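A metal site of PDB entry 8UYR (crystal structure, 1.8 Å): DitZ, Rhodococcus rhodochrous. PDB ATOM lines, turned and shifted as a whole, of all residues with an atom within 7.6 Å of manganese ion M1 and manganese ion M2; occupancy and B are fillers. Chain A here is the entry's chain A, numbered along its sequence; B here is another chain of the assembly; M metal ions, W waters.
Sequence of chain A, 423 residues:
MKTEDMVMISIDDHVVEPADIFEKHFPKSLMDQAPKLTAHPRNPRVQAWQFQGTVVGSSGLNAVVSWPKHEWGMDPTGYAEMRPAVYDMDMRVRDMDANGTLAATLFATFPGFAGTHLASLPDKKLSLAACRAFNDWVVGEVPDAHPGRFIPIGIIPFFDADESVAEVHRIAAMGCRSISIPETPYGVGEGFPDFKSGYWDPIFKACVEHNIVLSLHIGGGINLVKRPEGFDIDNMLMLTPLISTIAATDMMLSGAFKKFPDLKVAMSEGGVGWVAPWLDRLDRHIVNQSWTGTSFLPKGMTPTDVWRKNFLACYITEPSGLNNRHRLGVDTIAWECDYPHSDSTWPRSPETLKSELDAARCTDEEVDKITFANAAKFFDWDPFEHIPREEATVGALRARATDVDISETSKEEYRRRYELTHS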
ATOM      1  N   ILE A  11      26.752  -9.529  -8.053  1.00  0.00           N
ATOM      2  CA  ILE A  11      27.196  -8.136  -8.235  1.00  0.00           C
ATOM      3  C   ILE A  11      27.805  -7.924  -9.625  1.00  0.00           C
ATOM      4  O   ILE A  11      28.523  -6.954  -9.848  1.00  0.00           O
ATOM      5  CB  ILE A  11      28.150  -7.669  -7.118  1.00  0.00           C
ATOM      6  CG1 ILE A  11      29.094  -8.775  -6.678  1.00  0.00           C
ATOM      7  CG2 ILE A  11      27.351  -7.088  -5.915  1.00  0.00           C
ATOM      8  CD1 ILE A  11      30.136  -9.076  -7.692  1.00  0.00           C
ATOM      9  N   ASP A  12      27.489  -8.794 -10.593  1.00  0.00           N
ATOM     10  CA  ASP A  12      27.896  -8.556 -11.970  1.00  0.00           C
ATOM     11  C   ASP A  12      26.961  -9.356 -12.868  1.00  0.00           C
ATOM     12  O   ASP A  12      27.070 -10.584 -12.931  1.00  0.00           O
ATOM     13  CB  ASP A  12      29.361  -8.951 -12.171  1.00  0.00           C
ATOM     14  CG  ASP A  12      29.764  -8.989 -13.639  1.00  0.00           C
ATOM     15  OD1 ASP A  12      29.103  -8.326 -14.468  1.00  0.00           O
ATOM     16  OD2 ASP A  12      30.771  -9.660 -13.957  1.00  0.00           O
ATOM     17  N   ASP A  13      26.056  -8.657 -13.547  1.00  0.00           N
ATOM     18  CA  ASP A  13      25.287  -9.204 -14.659  1.00  0.00           C
ATOM     19  C   ASP A  13      25.276  -8.171 -15.757  1.00  0.00           C
ATOM     20  O   ASP A  13      25.840  -7.078 -15.615  1.00  0.00           O
ATOM     21  CB  ASP A  13      23.884  -9.585 -14.205  1.00  0.00           C
ATOM     22  CG  ASP A  13      23.897 -10.560 -13.055  1.00  0.00           C
ATOM     23  OD1 ASP A  13      24.014 -10.096 -11.903  1.00  0.00           O
ATOM     24  OD2 ASP A  13      23.850 -11.784 -13.305  1.00  0.00           O
ATOM     25  N   HIS A  14      24.613  -8.487 -16.857  1.00  0.00           N
ATOM     26  CA  HIS A  14      24.586  -7.616 -18.017  1.00  0.00           C
ATOM     27  C   HIS A  14      23.163  -7.481 -18.524  1.00  0.00           C
ATOM     28  O   HIS A  14      22.346  -8.393 -18.368  1.00  0.00           O
ATOM     29  CB  HIS A  14      25.541  -8.150 -19.083  1.00  0.00           C
ATOM     30  CG  HIS A  14      26.973  -8.169 -18.647  1.00  0.00           C
ATOM     31  ND1 HIS A  14      27.839  -7.140 -18.923  1.00  0.00           N
ATOM     32  CD2 HIS A  14      27.673  -9.070 -17.927  1.00  0.00           C
ATOM     33  CE1 HIS A  14      29.025  -7.412 -18.401  1.00  0.00           C
ATOM     34  NE2 HIS A  14      28.947  -8.581 -17.787  1.00  0.00           N
ATOM     35  N   LEU A  61      28.519 -13.732 -27.723  1.00  0.00           N
ATOM     36  CA  LEU A  61      28.953 -14.425 -26.510  1.00  0.00           C
ATOM     37  C   LEU A  61      28.327 -13.818 -25.265  1.00  0.00           C
ATOM     38  O   LEU A  61      28.546 -14.329 -24.158  1.00  0.00           O
ATOM     39  CB  LEU A  61      30.474 -14.411 -26.366  1.00  0.00           C
ATOM     40  CG  LEU A  61      31.298 -15.132 -27.422  1.00  0.00           C
ATOM     41  CD1 LEU A  61      32.783 -14.916 -27.136  1.00  0.00           C
ATOM     42  CD2 LEU A  61      30.953 -16.618 -27.493  1.00  0.00           C
ATOM     43  N   ASN A  62      27.579 -12.737 -25.413  1.00  0.00           N
ATOM     44  CA  ASN A  62      27.115 -11.963 -24.271  1.00  0.00           C
ATOM     45  C   ASN A  62      25.627 -12.107 -24.006  1.00  0.00           C
ATOM     46  O   ASN A  62      25.114 -11.494 -23.075  1.00  0.00           O
ATOM     47  CB  ASN A  62      27.483 -10.493 -24.475  1.00  0.00           C
ATOM     48  CG  ASN A  62      28.975 -10.247 -24.321  1.00  0.00           C
ATOM     49  OD1 ASN A  62      29.701 -11.105 -23.825  1.00  0.00           O
ATOM     50  ND2 ASN A  62      29.432  -9.069 -24.752  1.00  0.00           N
ATOM     51  N   THR A 105      23.059  -7.116 -10.761  1.00  0.00           N
ATOM     52  CA  THR A 105      23.719  -5.823 -10.900  1.00  0.00           C
ATOM     53  C   THR A 105      23.990  -5.605 -12.388  1.00  0.00           C
ATOM     54  O   THR A 105      24.875  -6.255 -12.953  1.00  0.00           O
ATOM     55  CB  THR A 105      25.017  -5.790 -10.090  1.00  0.00           C
ATOM     56  OG1 THR A 105      24.739  -6.136  -8.725  1.00  0.00           O
ATOM     57  CG2 THR A 105      25.664  -4.433 -10.109  1.00  0.00           C
ATOM     58  N   PHE A 107      25.182  -4.356 -15.759  1.00  0.00           N
ATOM     59  CA  PHE A 107      26.121  -3.603 -16.581  1.00  0.00           C
ATOM     60  C   PHE A 107      25.557  -3.363 -17.986  1.00  0.00           C
ATOM     61  O   PHE A 107      24.928  -4.253 -18.570  1.00  0.00           O
ATOM     62  CB  PHE A 107      27.467  -4.327 -16.681  1.00  0.00           C
ATOM     63  CG  PHE A 107      28.335  -4.207 -15.448  1.00  0.00           C
ATOM     64  CD1 PHE A 107      28.171  -5.060 -14.373  1.00  0.00           C
ATOM     65  CD2 PHE A 107      29.310  -3.229 -15.359  1.00  0.00           C
ATOM     66  CE1 PHE A 107      28.951  -4.937 -13.241  1.00  0.00           C
ATOM     67  CE2 PHE A 107      30.091  -3.111 -14.243  1.00  0.00           C
ATOM     68  CZ  PHE A 107      29.922  -3.962 -13.181  1.00  0.00           C
ATOM     69  N   PHE A 113      29.855  -1.292 -21.175  1.00  0.00           N
ATOM     70  CA  PHE A 113      29.598  -1.523 -19.748  1.00  0.00           C
ATOM     71  C   PHE A 113      30.266  -0.467 -18.872  1.00  0.00           C
ATOM     72  O   PHE A 113      29.891  -0.303 -17.715  1.00  0.00           O
ATOM     73  CB  PHE A 113      30.060  -2.914 -19.330  1.00  0.00           C
ATOM     74  CG  PHE A 113      31.456  -3.249 -19.752  1.00  0.00           C
ATOM     75  CD1 PHE A 113      32.548  -2.754 -19.058  1.00  0.00           C
ATOM     76  CD2 PHE A 113      31.674  -4.057 -20.858  1.00  0.00           C
ATOM     77  CE1 PHE A 113      33.844  -3.039 -19.462  1.00  0.00           C
ATOM     78  CE2 PHE A 113      32.970  -4.359 -21.263  1.00  0.00           C
ATOM     79  CZ  PHE A 113      34.054  -3.848 -20.556  1.00  0.00           C
ATOM     80  N   HIS A 217      35.109  -3.439 -14.278  1.00  0.00           N
ATOM     81  CA  HIS A 217      34.774  -4.683 -14.961  1.00  0.00           C
ATOM     82  C   HIS A 217      35.852  -5.065 -15.975  1.00  0.00           C
ATOM     83  O   HIS A 217      36.440  -4.189 -16.638  1.00  0.00           O
ATOM     84  CB  HIS A 217      33.436  -4.536 -15.660  1.00  0.00           C
ATOM     85  CG  HIS A 217      32.827  -5.827 -16.109  1.00  0.00           C
ATOM     86  ND1 HIS A 217      33.273  -6.523 -17.213  1.00  0.00           N
ATOM     87  CD2 HIS A 217      31.769  -6.538 -15.635  1.00  0.00           C
ATOM     88  CE1 HIS A 217      32.541  -7.609 -17.381  1.00  0.00           C
ATOM     89  NE2 HIS A 217      31.625  -7.644 -16.429  1.00  0.00           N
ATOM     90  N   ILE A 218      36.131  -6.368 -16.097  1.00  0.00           N
ATOM     91  CA  ILE A 218      37.113  -6.846 -17.084  1.00  0.00           C
ATOM     92  C   ILE A 218      36.701  -6.424 -18.501  1.00  0.00           C
ATOM     93  O   ILE A 218      35.525  -6.150 -18.795  1.00  0.00           O
ATOM     94  CB  ILE A 218      37.272  -8.369 -17.025  1.00  0.00           C
ATOM     95  CG1 ILE A 218      35.997  -9.037 -17.544  1.00  0.00           C
ATOM     96  CG2 ILE A 218      37.592  -8.826 -15.609  1.00  0.00           C
ATOM     97  CD1 ILE A 218      36.094 -10.559 -17.636  1.00  0.00           C
ATOM     98  N   PRO A 241      39.684 -12.681 -18.579  1.00  0.00           N
ATOM     99  CA  PRO A 241      39.301 -12.540 -17.164  1.00  0.00           C
ATOM    100  C   PRO A 241      40.407 -12.849 -16.168  1.00  0.00           C
ATOM    101  O   PRO A 241      40.119 -12.857 -14.963  1.00  0.00           O
ATOM    102  CB  PRO A 241      38.167 -13.545 -17.031  1.00  0.00           C
ATOM    103  CG  PRO A 241      38.577 -14.659 -17.954  1.00  0.00           C
ATOM    104  CD  PRO A 241      39.268 -13.998 -19.108  1.00  0.00           C
ATOM    105  N   SER A 268      35.049  -6.310 -10.836  1.00  0.00           N
ATOM    106  CA  SER A 268      33.939  -7.085 -11.376  1.00  0.00           C
ATOM    107  C   SER A 268      34.400  -8.094 -12.429  1.00  0.00           C
ATOM    108  O   SER A 268      35.137  -7.749 -13.359  1.00  0.00           O
ATOM    109  CB  SER A 268      32.904  -6.135 -11.960  1.00  0.00           C
ATOM    110  OG  SER A 268      32.687  -5.053 -11.055  1.00  0.00           O
ATOM    111  N   GLU A 269      33.959  -9.334 -12.273  1.00  0.00           N
ATOM    112  CA  GLU A 269      34.295 -10.462 -13.165  1.00  0.00           C
ATOM    113  C   GLU A 269      35.790 -10.775 -13.186  1.00  0.00           C
ATOM    114  O   GLU A 269      36.279 -11.460 -14.090  1.00  0.00           O
ATOM    115  CB  GLU A 269      33.785 -10.236 -14.602  1.00  0.00           C
ATOM    116  CG  GLU A 269      33.371 -11.598 -15.276  1.00  0.00           C
ATOM    117  CD  GLU A 269      32.718 -11.483 -16.653  1.00  0.00           C
ATOM    118  OE1 GLU A 269      31.932 -10.543 -16.913  1.00  0.00           O
ATOM    119  OE2 GLU A 269      32.979 -12.378 -17.498  1.00  0.00           O
ATOM    120  N   GLY A 270      36.528 -10.329 -12.177  1.00  0.00           N
ATOM    121  CA  GLY A 270      37.950 -10.574 -12.175  1.00  0.00           C
ATOM    122  C   GLY A 270      38.398 -11.901 -11.637  1.00  0.00           C
ATOM    123  O   GLY A 270      39.556 -12.271 -11.824  1.00  0.00           O
ATOM    124  N   ILE A 316      32.484 -15.924 -10.558  1.00  0.00           N
ATOM    125  CA  ILE A 316      31.355 -16.767 -10.933  1.00  0.00           C
ATOM    126  C   ILE A 316      31.588 -18.179 -10.439  1.00  0.00           C
ATOM    127  O   ILE A 316      30.786 -18.762  -9.694  1.00  0.00           O
ATOM    128  CB  ILE A 316      31.174 -16.780 -12.459  1.00  0.00           C
ATOM    129  CG1 ILE A 316      31.141 -15.355 -13.025  1.00  0.00           C
ATOM    130  CG2 ILE A 316      29.919 -17.554 -12.842  1.00  0.00           C
ATOM    131  CD1 ILE A 316      31.399 -15.326 -14.532  1.00  0.00           C
ATOM    132  N   GLU A 336      29.047 -13.731  -8.281  1.00  0.00           N
ATOM    133  CA  GLU A 336      28.291 -13.088  -9.348  1.00  0.00           C
ATOM    134  C   GLU A 336      27.810 -14.151 -10.315  1.00  0.00           C
ATOM    135  O   GLU A 336      28.435 -15.201 -10.459  1.00  0.00           O
ATOM    136  CB  GLU A 336      29.124 -12.052 -10.098  1.00  0.00           C
ATOM    137  CG  GLU A 336      30.466 -12.582 -10.481  1.00  0.00           C
ATOM    138  CD  GLU A 336      31.158 -11.660 -11.451  1.00  0.00           C
ATOM    139  OE1 GLU A 336      30.921 -11.806 -12.661  1.00  0.00           O
ATOM    140  OE2 GLU A 336      31.886 -10.770 -10.988  1.00  0.00           O
ATOM    141  N   CYS A 337      26.708 -13.839 -11.018  1.00  0.00           N
ATOM    142  CA  CYS A 337      26.126 -14.777 -11.969  1.00  0.00           C
ATOM    143  C   CYS A 337      26.597 -14.539 -13.404  1.00  0.00           C
ATOM    144  O   CYS A 337      26.748 -15.501 -14.161  1.00  0.00           O
ATOM    145  CB  CYS A 337      24.600 -14.669 -11.929  1.00  0.00           C
ATOM    146  SG  CYS A 337      23.747 -15.962 -12.883  1.00  0.00           S
ATOM    147  N   ASP A 338      26.791 -13.269 -13.774  1.00  0.00           N
ATOM    148  CA  ASP A 338      27.210 -12.837 -15.115  1.00  0.00           C
ATOM    149  C   ASP A 338      26.181 -13.205 -16.182  1.00  0.00           C
ATOM    150  O   ASP A 338      26.528 -13.404 -17.345  1.00  0.00           O
ATOM    151  CB  ASP A 338      28.586 -13.368 -15.482  1.00  0.00           C
ATOM    152  CG  ASP A 338      29.328 -12.434 -16.449  1.00  0.00           C
ATOM    153  OD1 ASP A 338      29.168 -11.195 -16.316  1.00  0.00           O
ATOM    154  OD2 ASP A 338      30.043 -12.963 -17.339  1.00  0.00           O
ATOM    155  N   TYR A 339      24.928 -13.295 -15.791  1.00  0.00           N
ATOM    156  CA  TYR A 339      23.844 -13.488 -16.741  1.00  0.00           C
ATOM    157  C   TYR A 339      23.789 -12.300 -17.698  1.00  0.00           C
ATOM    158  O   TYR A 339      23.916 -11.150 -17.265  1.00  0.00           O
ATOM    159  CB  TYR A 339      22.534 -13.621 -15.957  1.00  0.00           C
ATOM    160  CG  TYR A 339      21.299 -13.897 -16.770  1.00  0.00           C
ATOM    161  CD1 TYR A 339      20.753 -12.927 -17.598  1.00  0.00           C
ATOM    162  CD2 TYR A 339      20.637 -15.128 -16.671  1.00  0.00           C
ATOM    163  CE1 TYR A 339      19.610 -13.162 -18.340  1.00  0.00           C
ATOM    164  CE2 TYR A 339      19.487 -15.369 -17.418  1.00  0.00           C
ATOM    165  CZ  TYR A 339      18.983 -14.382 -18.240  1.00  0.00           C
ATOM    166  OH  TYR A 339      17.833 -14.595 -18.976  1.00  0.00           O
ATOM    167  N   PRO A 340      23.612 -12.529 -19.013  1.00  0.00           N
ATOM    168  CA  PRO A 340      23.464 -13.777 -19.770  1.00  0.00           C
ATOM    169  C   PRO A 340      24.716 -14.143 -20.565  1.00  0.00           C
ATOM    170  O   PRO A 340      24.607 -14.693 -21.659  1.00  0.00           O
ATOM    171  CB  PRO A 340      22.303 -13.443 -20.725  1.00  0.00           C
ATOM    172  CG  PRO A 340      22.372 -11.901 -20.914  1.00  0.00           C
ATOM    173  CD  PRO A 340      23.369 -11.357 -19.872  1.00  0.00           C
ATOM    174  N   HIS A 341      25.888 -13.843 -20.017  1.00  0.00           N
ATOM    175  CA  HIS A 341      27.143 -14.079 -20.701  1.00  0.00           C
ATOM    176  C   HIS A 341      27.454 -15.565 -20.791  1.00  0.00           C
ATOM    177  O   HIS A 341      26.973 -16.382 -19.999  1.00  0.00           O
ATOM    178  CB  HIS A 341      28.303 -13.401 -19.975  1.00  0.00           C
ATOM    179  CG  HIS A 341      28.451 -11.944 -20.307  1.00  0.00           C
ATOM    180  ND1 HIS A 341      29.594 -11.233 -20.005  1.00  0.00           N
ATOM    181  CD2 HIS A 341      27.608 -11.073 -20.897  1.00  0.00           C
ATOM    182  CE1 HIS A 341      29.443  -9.981 -20.402  1.00  0.00           C
ATOM    183  NE2 HIS A 341      28.250  -9.853 -20.942  1.00  0.00           N
ATOM    184  N   SER A 342      28.327 -15.894 -21.756  1.00  0.00           N
ATOM    185  CA  SER A 342      28.839 -17.250 -21.923  1.00  0.00           C
ATOM    186  C   SER A 342      29.406 -17.833 -20.628  1.00  0.00           C
ATOM    187  O   SER A 342      29.337 -19.052 -20.425  1.00  0.00           O
ATOM    188  CB  SER A 342      29.905 -17.242 -23.014  1.00  0.00           C
ATOM    189  OG  SER A 342      30.859 -16.211 -22.802  1.00  0.00           O
ATOM    190  N   ASP A 343      29.961 -17.004 -19.760  1.00  0.00           N
ATOM    191  CA  ASP A 343      30.549 -17.502 -18.521  1.00  0.00           C
ATOM    192  C   ASP A 343      29.544 -17.737 -17.407  1.00  0.00           C
ATOM    193  O   ASP A 343      29.907 -18.338 -16.387  1.00  0.00           O
ATOM    194  CB  ASP A 343      31.638 -16.529 -18.039  1.00  0.00           C
ATOM    195  CG  ASP A 343      32.904 -16.600 -18.884  1.00  0.00           C
ATOM    196  OD1 ASP A 343      33.583 -17.645 -18.819  1.00  0.00           O
ATOM    197  OD2 ASP A 343      33.201 -15.633 -19.620  1.00  0.00           O
ATOM    198  N   SER A 344      28.282 -17.326 -17.566  1.00  0.00           N
ATOM    199  CA  SER A 344      27.298 -17.509 -16.512  1.00  0.00           C
ATOM    200  C   SER A 344      27.071 -18.991 -16.170  1.00  0.00           C
ATOM    201  O   SER A 344      27.149 -19.869 -17.033  1.00  0.00           O
ATOM    202  CB  SER A 344      25.971 -16.891 -16.910  1.00  0.00           C
ATOM    203  OG  SER A 344      25.024 -17.033 -15.868  1.00  0.00           O
ATOM    204  N   ARG B 281      40.195 -22.236 -15.164  1.00  0.00           N
ATOM    205  CA  ARG B 281      39.549 -21.758 -16.387  1.00  0.00           C
ATOM    206  C   ARG B 281      39.839 -22.668 -17.573  1.00  0.00           C
ATOM    207  O   ARG B 281      38.954 -22.918 -18.391  1.00  0.00           O
ATOM    208  CB  ARG B 281      39.977 -20.325 -16.683  1.00  0.00           C
ATOM    209  CG  ARG B 281      39.150 -19.734 -17.817  1.00  0.00           C
ATOM    210  CD  ARG B 281      39.304 -18.232 -17.938  1.00  0.00           C
ATOM    211  NE  ARG B 281      38.488 -17.754 -19.048  1.00  0.00           N
ATOM    212  CZ  ARG B 281      37.173 -17.589 -18.988  1.00  0.00           C
ATOM    213  NH1 ARG B 281      36.506 -17.836 -17.847  1.00  0.00           N
ATOM    214  NH2 ARG B 281      36.516 -17.159 -20.056  1.00  0.00           N
HETATM  215 MN    MN M   1      31.243 -11.966 -18.781  1.00  0.00          MN
HETATM  216 MN    MN M   2      30.277  -9.339 -16.184  1.00  0.00          MN
HETATM  217  O   HOH W   1      31.586 -13.718 -20.010  1.00  0.00           O
HETATM  218  O   HOH W   2      32.572 -10.689 -19.838  1.00  0.00           O
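Manganese ion M2 is bound by the side-chain carboxylate (OD1) of Asp 338 (2.2 Å), the side-chain carboxylate (OE1) of Glu 269 (2.2 Å), a ring nitrogen (NE2) of His 217 (2.2 Å), a ring nitrogen (NE2) of His 14 (2.2 Å), the side-chain carboxylate (OD2) of Asp 12 (2.3 Å) and the side-chain carboxylate (OD1) of Asp 12 (2.3 Å).
Manganese ion M2 has six donor atoms within binding distance.
Within 4 Å of manganese ion M2: Asp 12, His 14, His 217, Glu 269 and Asp 338.
N of Asp 338 sits at hydrogen-bond distance from OD2 of Asp 13 (3.3 Å).
N of Glu 269 lies within hydrogen-bond range of OE2 of Glu 336, 2.8 Å away.
A ring nitrogen (NE2) of His 341 sits close to a ring nitrogen (ND1) of His 14 (3.4 Å).
The side-chain amide oxygen (OD1) of Asn 62 lies within hydrogen-bond range of a ring nitrogen (NE2) of His 341 (3.5 Å).
N of His 14 sits at hydrogen-bond distance from O of Tyr 339.
The side-chain carboxylate of Asp 12 lies close to the side-chain carboxylate of Glu 336 (2.5 Å).
Manganese ion M1 is bound by water W2 (2.1 Å), the side-chain carboxylate (OD2) of Asp 338 (2.1 Å), water W1 (2.2 Å), a ring nitrogen (ND1) of His 341 (2.2 Å), the side-chain carboxylate (OE2) of Glu 269 (2.2 Å) and the side-chain carboxylate (OE1) of Glu 269 (2.4 Å).
Manganese ion M1 has six donor atoms within binding distance.
Three residues have an atom within 4 Å of manganese ion M1: Glu 269, Asp 338 and His 341.
The nearest printed residue that does not touch manganese ion M1 is His 14 (4.2 Å).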
